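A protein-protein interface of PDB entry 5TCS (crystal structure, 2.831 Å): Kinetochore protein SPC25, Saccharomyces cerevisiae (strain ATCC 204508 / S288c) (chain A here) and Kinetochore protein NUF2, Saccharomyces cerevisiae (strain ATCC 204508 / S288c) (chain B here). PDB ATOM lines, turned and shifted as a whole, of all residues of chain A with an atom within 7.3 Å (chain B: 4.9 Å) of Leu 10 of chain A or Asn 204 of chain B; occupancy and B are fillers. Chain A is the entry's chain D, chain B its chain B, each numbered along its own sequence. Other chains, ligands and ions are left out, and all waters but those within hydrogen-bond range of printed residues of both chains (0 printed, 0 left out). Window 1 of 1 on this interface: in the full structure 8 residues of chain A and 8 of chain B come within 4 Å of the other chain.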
ATOM      1  N   ALA A   6     -13.765  -2.560  15.014  1.00  0.00           N
ATOM      2  CA  ALA A   6     -13.093  -3.829  15.256  1.00  0.00           C
ATOM      3  C   ALA A   6     -13.945  -5.033  14.869  1.00  0.00           C
ATOM      4  O   ALA A   6     -13.546  -6.169  15.147  1.00  0.00           O
ATOM      5  CB  ALA A   6     -12.693  -3.937  16.729  1.00  0.00           C
ATOM      6  N   PHE A   7     -15.099  -4.811  14.233  1.00  0.00           N
ATOM      7  CA  PHE A   7     -15.972  -5.927  13.885  1.00  0.00           C
ATOM      8  C   PHE A   7     -15.260  -6.937  13.000  1.00  0.00           C
ATOM      9  O   PHE A   7     -15.540  -8.139  13.083  1.00  0.00           O
ATOM     10  CB  PHE A   7     -17.230  -5.417  13.188  1.00  0.00           C
ATOM     11  CG  PHE A   7     -18.237  -6.490  12.911  1.00  0.00           C
ATOM     12  CD1 PHE A   7     -18.808  -7.199  13.955  1.00  0.00           C
ATOM     13  CD2 PHE A   7     -18.612  -6.794  11.614  1.00  0.00           C
ATOM     14  CE1 PHE A   7     -19.732  -8.192  13.711  1.00  0.00           C
ATOM     15  CE2 PHE A   7     -19.539  -7.784  11.365  1.00  0.00           C
ATOM     16  CZ  PHE A   7     -20.101  -8.483  12.417  1.00  0.00           C
ATOM     17  N   SER A   8     -14.347  -6.472  12.143  1.00  0.00           N
ATOM     18  CA  SER A   8     -13.507  -7.387  11.380  1.00  0.00           C
ATOM     19  C   SER A   8     -13.025  -8.526  12.266  1.00  0.00           C
ATOM     20  O   SER A   8     -13.257  -9.703  11.969  1.00  0.00           O
ATOM     21  CB  SER A   8     -12.324  -6.623  10.781  1.00  0.00           C
ATOM     22  OG  SER A   8     -11.683  -5.829  11.765  1.00  0.00           O
ATOM     23  N   ASP A   9     -12.389  -8.185  13.391  1.00  0.00           N
ATOM     24  CA  ASP A   9     -11.866  -9.201  14.296  1.00  0.00           C
ATOM     25  C   ASP A   9     -12.920 -10.251  14.612  1.00  0.00           C
ATOM     26  O   ASP A   9     -12.666 -11.456  14.504  1.00  0.00           O
ATOM     27  CB  ASP A   9     -11.361  -8.546  15.584  1.00  0.00           C
ATOM     28  CG  ASP A   9     -10.135  -7.681  15.360  1.00  0.00           C
ATOM     29  OD1 ASP A   9      -9.521  -7.783  14.275  1.00  0.00           O
ATOM     30  OD2 ASP A   9      -9.778  -6.904  16.271  1.00  0.00           O
ATOM     31  N   LEU A  10     -14.119  -9.815  14.998  1.00  0.00           N
ATOM     32  CA  LEU A  10     -15.142 -10.781  15.379  1.00  0.00           C
ATOM     33  C   LEU A  10     -15.485 -11.699  14.212  1.00  0.00           C
ATOM     34  O   LEU A  10     -15.630 -12.914  14.391  1.00  0.00           O
ATOM     35  CB  LEU A  10     -16.389 -10.059  15.893  1.00  0.00           C
ATOM     36  CG  LEU A  10     -17.318 -10.885  16.792  1.00  0.00           C
ATOM     37  CD1 LEU A  10     -16.594 -11.405  18.032  1.00  0.00           C
ATOM     38  CD2 LEU A  10     -18.530 -10.062  17.204  1.00  0.00           C
ATOM     39  N   GLU A  11     -15.575 -11.143  12.999  1.00  0.00           N
ATOM     40  CA  GLU A  11     -15.880 -11.974  11.838  1.00  0.00           C
ATOM     41  C   GLU A  11     -14.910 -13.139  11.722  1.00  0.00           C
ATOM     42  O   GLU A  11     -15.270 -14.196  11.192  1.00  0.00           O
ATOM     43  CB  GLU A  11     -15.854 -11.142  10.554  1.00  0.00           C
ATOM     44  CG  GLU A  11     -16.918 -10.058  10.484  1.00  0.00           C
ATOM     45  CD  GLU A  11     -17.276  -9.687   9.057  1.00  0.00           C
ATOM     46  OE1 GLU A  11     -17.999 -10.467   8.403  1.00  0.00           O
ATOM     47  OE2 GLU A  11     -16.825  -8.620   8.587  1.00  0.00           O
ATOM     48  N   ARG A  12     -13.678 -12.974  12.209  1.00  0.00           N
ATOM     49  CA  ARG A  12     -12.751 -14.096  12.255  1.00  0.00           C
ATOM     50  C   ARG A  12     -13.315 -15.182  13.159  1.00  0.00           C
ATOM     51  O   ARG A  12     -13.656 -16.272  12.690  1.00  0.00           O
ATOM     52  CB  ARG A  12     -11.369 -13.650  12.744  1.00  0.00           C
ATOM     53  CG  ARG A  12     -10.395 -13.279  11.633  1.00  0.00           C
ATOM     54  CD  ARG A  12      -9.226 -12.451  12.164  1.00  0.00           C
ATOM     55  NE  ARG A  12      -8.090 -13.271  12.579  1.00  0.00           N
ATOM     56  CZ  ARG A  12      -7.044 -12.812  13.259  1.00  0.00           C
ATOM     57  NH1 ARG A  12      -6.988 -11.534  13.618  1.00  0.00           N
ATOM     58  NH2 ARG A  12      -6.052 -13.628  13.590  1.00  0.00           N
ATOM     59  N   ARG A  13     -13.448 -14.880  14.454  1.00  0.00           N
ATOM     60  CA  ARG A  13     -13.866 -15.894  15.416  1.00  0.00           C
ATOM     61  C   ARG A  13     -15.141 -16.589  14.959  1.00  0.00           C
ATOM     62  O   ARG A  13     -15.229 -17.824  14.968  1.00  0.00           O
ATOM     63  CB  ARG A  13     -14.073 -15.265  16.796  1.00  0.00           C
ATOM     64  CG  ARG A  13     -12.796 -14.780  17.462  1.00  0.00           C
ATOM     65  CD  ARG A  13     -12.893 -14.911  18.975  1.00  0.00           C
ATOM     66  NE  ARG A  13     -11.875 -14.115  19.664  1.00  0.00           N
ATOM     67  CZ  ARG A  13     -12.117 -13.078  20.464  1.00  0.00           C
ATOM     68  NH1 ARG A  13     -13.359 -12.681  20.718  1.00  0.00           N
ATOM     69  NH2 ARG A  13     -11.103 -12.435  21.029  1.00  0.00           N
ATOM     70  N   MET A  14     -16.134 -15.811  14.545  1.00  0.00           N
ATOM     71  CA  MET A  14     -17.392 -16.369  14.073  1.00  0.00           C
ATOM     72  C   MET A  14     -17.143 -17.359  12.940  1.00  0.00           C
ATOM     73  O   MET A  14     -17.592 -18.504  13.007  1.00  0.00           O
ATOM     74  CB  MET A  14     -18.334 -15.249  13.626  1.00  0.00           C
ATOM     75  CG  MET A  14     -19.044 -14.582  14.794  1.00  0.00           C
ATOM     76  SD  MET A  14     -19.753 -12.813  14.409  1.00  0.00           S
ATOM     77  CE  MET A  14     -21.451 -13.305  13.622  1.00  0.00           C
ATOM     78  N   ASP A  15     -16.398 -16.932  11.916  1.00  0.00           N
ATOM     79  CA  ASP A  15     -16.093 -17.840  10.816  1.00  0.00           C
ATOM     80  C   ASP A  15     -15.437 -19.117  11.322  1.00  0.00           C
ATOM     81  O   ASP A  15     -15.663 -20.196  10.763  1.00  0.00           O
ATOM     82  CB  ASP A  15     -15.194 -17.150   9.791  1.00  0.00           C
ATOM     83  CG  ASP A  15     -15.925 -16.078   9.005  1.00  0.00           C
ATOM     84  OD1 ASP A  15     -17.171 -16.134   8.942  1.00  0.00           O
ATOM     85  OD2 ASP A  15     -15.254 -15.184   8.445  1.00  0.00           O
ATOM     86  N   GLY A  16     -14.629 -19.019  12.380  1.00  0.00           N
ATOM     87  CA  GLY A  16     -14.075 -20.220  12.983  1.00  0.00           C
ATOM     88  C   GLY A  16     -15.136 -21.036  13.697  1.00  0.00           C
ATOM     89  O   GLY A  16     -15.244 -22.248  13.496  1.00  0.00           O
ATOM     90  N   TYR B 196     -23.694  -1.819  19.868  1.00  0.00           N
ATOM     91  CA  TYR B 196     -22.777  -2.768  19.251  1.00  0.00           C
ATOM     92  C   TYR B 196     -21.959  -3.498  20.301  1.00  0.00           C
ATOM     93  O   TYR B 196     -21.725  -4.702  20.184  1.00  0.00           O
ATOM     94  CB  TYR B 196     -21.834  -2.077  18.268  1.00  0.00           C
ATOM     95  CG  TYR B 196     -20.730  -3.010  17.818  1.00  0.00           C
ATOM     96  CD1 TYR B 196     -20.927  -3.893  16.764  1.00  0.00           C
ATOM     97  CD2 TYR B 196     -19.503  -3.035  18.471  1.00  0.00           C
ATOM     98  CE1 TYR B 196     -19.929  -4.760  16.360  1.00  0.00           C
ATOM     99  CE2 TYR B 196     -18.501  -3.900  18.077  1.00  0.00           C
ATOM    100  CZ  TYR B 196     -18.720  -4.760  17.020  1.00  0.00           C
ATOM    101  OH  TYR B 196     -17.722  -5.621  16.622  1.00  0.00           O
ATOM    102  N   SER B 200     -21.696  -7.493  20.717  1.00  0.00           N
ATOM    103  CA  SER B 200     -20.442  -8.237  20.714  1.00  0.00           C
ATOM    104  C   SER B 200     -20.321  -9.095  21.964  1.00  0.00           C
ATOM    105  O   SER B 200     -20.063 -10.300  21.881  1.00  0.00           O
ATOM    106  CB  SER B 200     -19.260  -7.270  20.610  1.00  0.00           C
ATOM    107  OG  SER B 200     -18.031  -7.935  20.855  1.00  0.00           O
ATOM    108  N   GLY B 201     -20.500  -8.489  23.139  1.00  0.00           N
ATOM    109  CA  GLY B 201     -20.494  -9.270  24.364  1.00  0.00           C
ATOM    110  C   GLY B 201     -21.484 -10.415  24.320  1.00  0.00           C
ATOM    111  O   GLY B 201     -21.197 -11.519  24.788  1.00  0.00           O
ATOM    112  N   HIS B 202     -22.662 -10.169  23.742  1.00  0.00           N
ATOM    113  CA  HIS B 202     -23.670 -11.216  23.620  1.00  0.00           C
ATOM    114  C   HIS B 202     -23.157 -12.375  22.774  1.00  0.00           C
ATOM    115  O   HIS B 202     -23.227 -13.538  23.186  1.00  0.00           O
ATOM    116  CB  HIS B 202     -24.946 -10.633  23.017  1.00  0.00           C
ATOM    117  CG  HIS B 202     -26.145 -11.515  23.171  1.00  0.00           C
ATOM    118  ND1 HIS B 202     -26.795 -11.685  24.375  1.00  0.00           N
ATOM    119  CD2 HIS B 202     -26.811 -12.279  22.274  1.00  0.00           C
ATOM    120  CE1 HIS B 202     -27.811 -12.513  24.212  1.00  0.00           C
ATOM    121  NE2 HIS B 202     -27.843 -12.889  22.946  1.00  0.00           N
ATOM    122  N   ILE B 203     -22.639 -12.075  21.582  1.00  0.00           N
ATOM    123  CA  ILE B 203     -22.169 -13.121  20.676  1.00  0.00           C
ATOM    124  C   ILE B 203     -21.015 -13.894  21.306  1.00  0.00           C
ATOM    125  O   ILE B 203     -20.995 -15.130  21.293  1.00  0.00           O
ATOM    126  CB  ILE B 203     -21.775 -12.504  19.320  1.00  0.00           C
ATOM    127  CG1 ILE B 203     -23.035 -12.216  18.498  1.00  0.00           C
ATOM    128  CG2 ILE B 203     -20.826 -13.419  18.541  1.00  0.00           C
ATOM    129  CD1 ILE B 203     -22.820 -11.251  17.348  1.00  0.00           C
ATOM    130  N   ASN B 204     -20.028 -13.178  21.849  1.00  0.00           N
ATOM    131  CA  ASN B 204     -18.909 -13.844  22.510  1.00  0.00           C
ATOM    132  C   ASN B 204     -19.401 -14.764  23.619  1.00  0.00           C
ATOM    133  O   ASN B 204     -18.939 -15.902  23.749  1.00  0.00           O
ATOM    134  CB  ASN B 204     -17.934 -12.807  23.069  1.00  0.00           C
ATOM    135  CG  ASN B 204     -16.952 -12.308  22.029  1.00  0.00           C
ATOM    136  OD1 ASN B 204     -16.090 -13.056  21.564  1.00  0.00           O
ATOM    137  ND2 ASN B 204     -17.070 -11.037  21.663  1.00  0.00           N
ATOM    138  N   LYS B 205     -20.335 -14.279  24.439  1.00  0.00           N
ATOM    139  CA  LYS B 205     -20.948 -15.120  25.461  1.00  0.00           C
ATOM    140  C   LYS B 205     -21.547 -16.375  24.839  1.00  0.00           C
ATOM    141  O   LYS B 205     -21.348 -17.492  25.332  1.00  0.00           O
ATOM    142  CB  LYS B 205     -22.020 -14.315  26.196  1.00  0.00           C
ATOM    143  CG  LYS B 205     -22.631 -14.996  27.402  1.00  0.00           C
ATOM    144  CD  LYS B 205     -23.727 -14.124  27.994  1.00  0.00           C
ATOM    145  CE  LYS B 205     -24.636 -14.906  28.923  1.00  0.00           C
ATOM    146  NZ  LYS B 205     -25.805 -14.090  29.358  1.00  0.00           N
ATOM    147  N   TYR B 206     -22.285 -16.199  23.742  1.00  0.00           N
ATOM    148  CA  TYR B 206     -22.893 -17.323  23.041  1.00  0.00           C
ATOM    149  C   TYR B 206     -21.849 -18.352  22.623  1.00  0.00           C
ATOM    150  O   TYR B 206     -22.058 -19.558  22.788  1.00  0.00           O
ATOM    151  CB  TYR B 206     -23.659 -16.792  21.829  1.00  0.00           C
ATOM    152  CG  TYR B 206     -24.094 -17.828  20.822  1.00  0.00           C
ATOM    153  CD1 TYR B 206     -25.189 -18.643  21.061  1.00  0.00           C
ATOM    154  CD2 TYR B 206     -23.424 -17.966  19.615  1.00  0.00           C
ATOM    155  CE1 TYR B 206     -25.595 -19.577  20.137  1.00  0.00           C
ATOM    156  CE2 TYR B 206     -23.821 -18.897  18.684  1.00  0.00           C
ATOM    157  CZ  TYR B 206     -24.908 -19.700  18.950  1.00  0.00           C
ATOM    158  OH  TYR B 206     -25.313 -20.632  18.023  1.00  0.00           O
ATOM    159  N   MET B 207     -20.720 -17.899  22.092  1.00  0.00           N
ATOM    160  CA  MET B 207     -19.694 -18.813  21.605  1.00  0.00           C
ATOM    161  C   MET B 207     -18.961 -19.497  22.757  1.00  0.00           C
ATOM    162  O   MET B 207     -18.551 -20.651  22.641  1.00  0.00           O
ATOM    163  CB  MET B 207     -18.701 -18.069  20.712  1.00  0.00           C
ATOM    164  CG  MET B 207     -19.272 -17.694  19.352  1.00  0.00           C
ATOM    165  SD  MET B 207     -17.926 -17.042  18.099  1.00  0.00           S
ATOM    166  CE  MET B 207     -17.428 -15.388  19.004  1.00  0.00           C
ATOM    167  N   ASN B 208     -18.799 -18.780  23.869  1.00  0.00           N
ATOM    168  CA  ASN B 208     -18.157 -19.368  25.041  1.00  0.00           C
ATOM    169  C   ASN B 208     -19.009 -20.487  25.625  1.00  0.00           C
ATOM    170  O   ASN B 208     -18.534 -21.615  25.805  1.00  0.00           O
ATOM    171  CB  ASN B 208     -17.894 -18.291  26.094  1.00  0.00           C
ATOM    172  CG  ASN B 208     -16.805 -17.325  25.683  1.00  0.00           C
ATOM    173  OD1 ASN B 208     -15.933 -17.658  24.879  1.00  0.00           O
ATOM    174  ND2 ASN B 208     -16.842 -16.119  26.239  1.00  0.00           N
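Of the printed residues of chain B, Phe 7 of chain A touches Tyr 196 (3.3 Å).
Of the printed residues of chain B, Arg 13 of chain A touches Asn 204.
Printed residues of chain A within 4 Å of Tyr 196 of chain B: Phe 7.
Asn 204 of chain B touches just these residues of chain A: Leu 10 (3.7 Å) and Arg 13 (2.9 Å).
The nearest printed residue of chain A that does not touch Tyr 196 of chain B is Ala 6 of chain A (4.2 Å).
Of the 11 printed residues of chain A, 3 touch a printed residue of chain B.
Printed residues of chain A that touch a printed residue of chain B: Phe 7, Leu 10 and Arg 13.
Hydrophobic or aromatic side chains of chain A that line the printed part of chain B: Phe 7 and Leu 10.
Among the printed residues, 3 pairs touch across the chains.
Among the printed residues, merely in contact across the chains: Phe 7 of chain A with Tyr 196 of chain B and Leu 10 of chain A with Asn 204 of chain B.
ND2 of Asn 204 of chain B lies within hydrogen-bond range of O of Ser 200 of chain B, 3.1 Å away.
The backbone carbonyl oxygen (O) of Asn 204 of chain B sits close to the side-chain amide nitrogen (ND2) of Asn 208 of chain B, 3.3 Å away.
OD1 of Asn 204 of chain B is in hydrogen-bond range of NH1 of Arg 13 of chain A.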
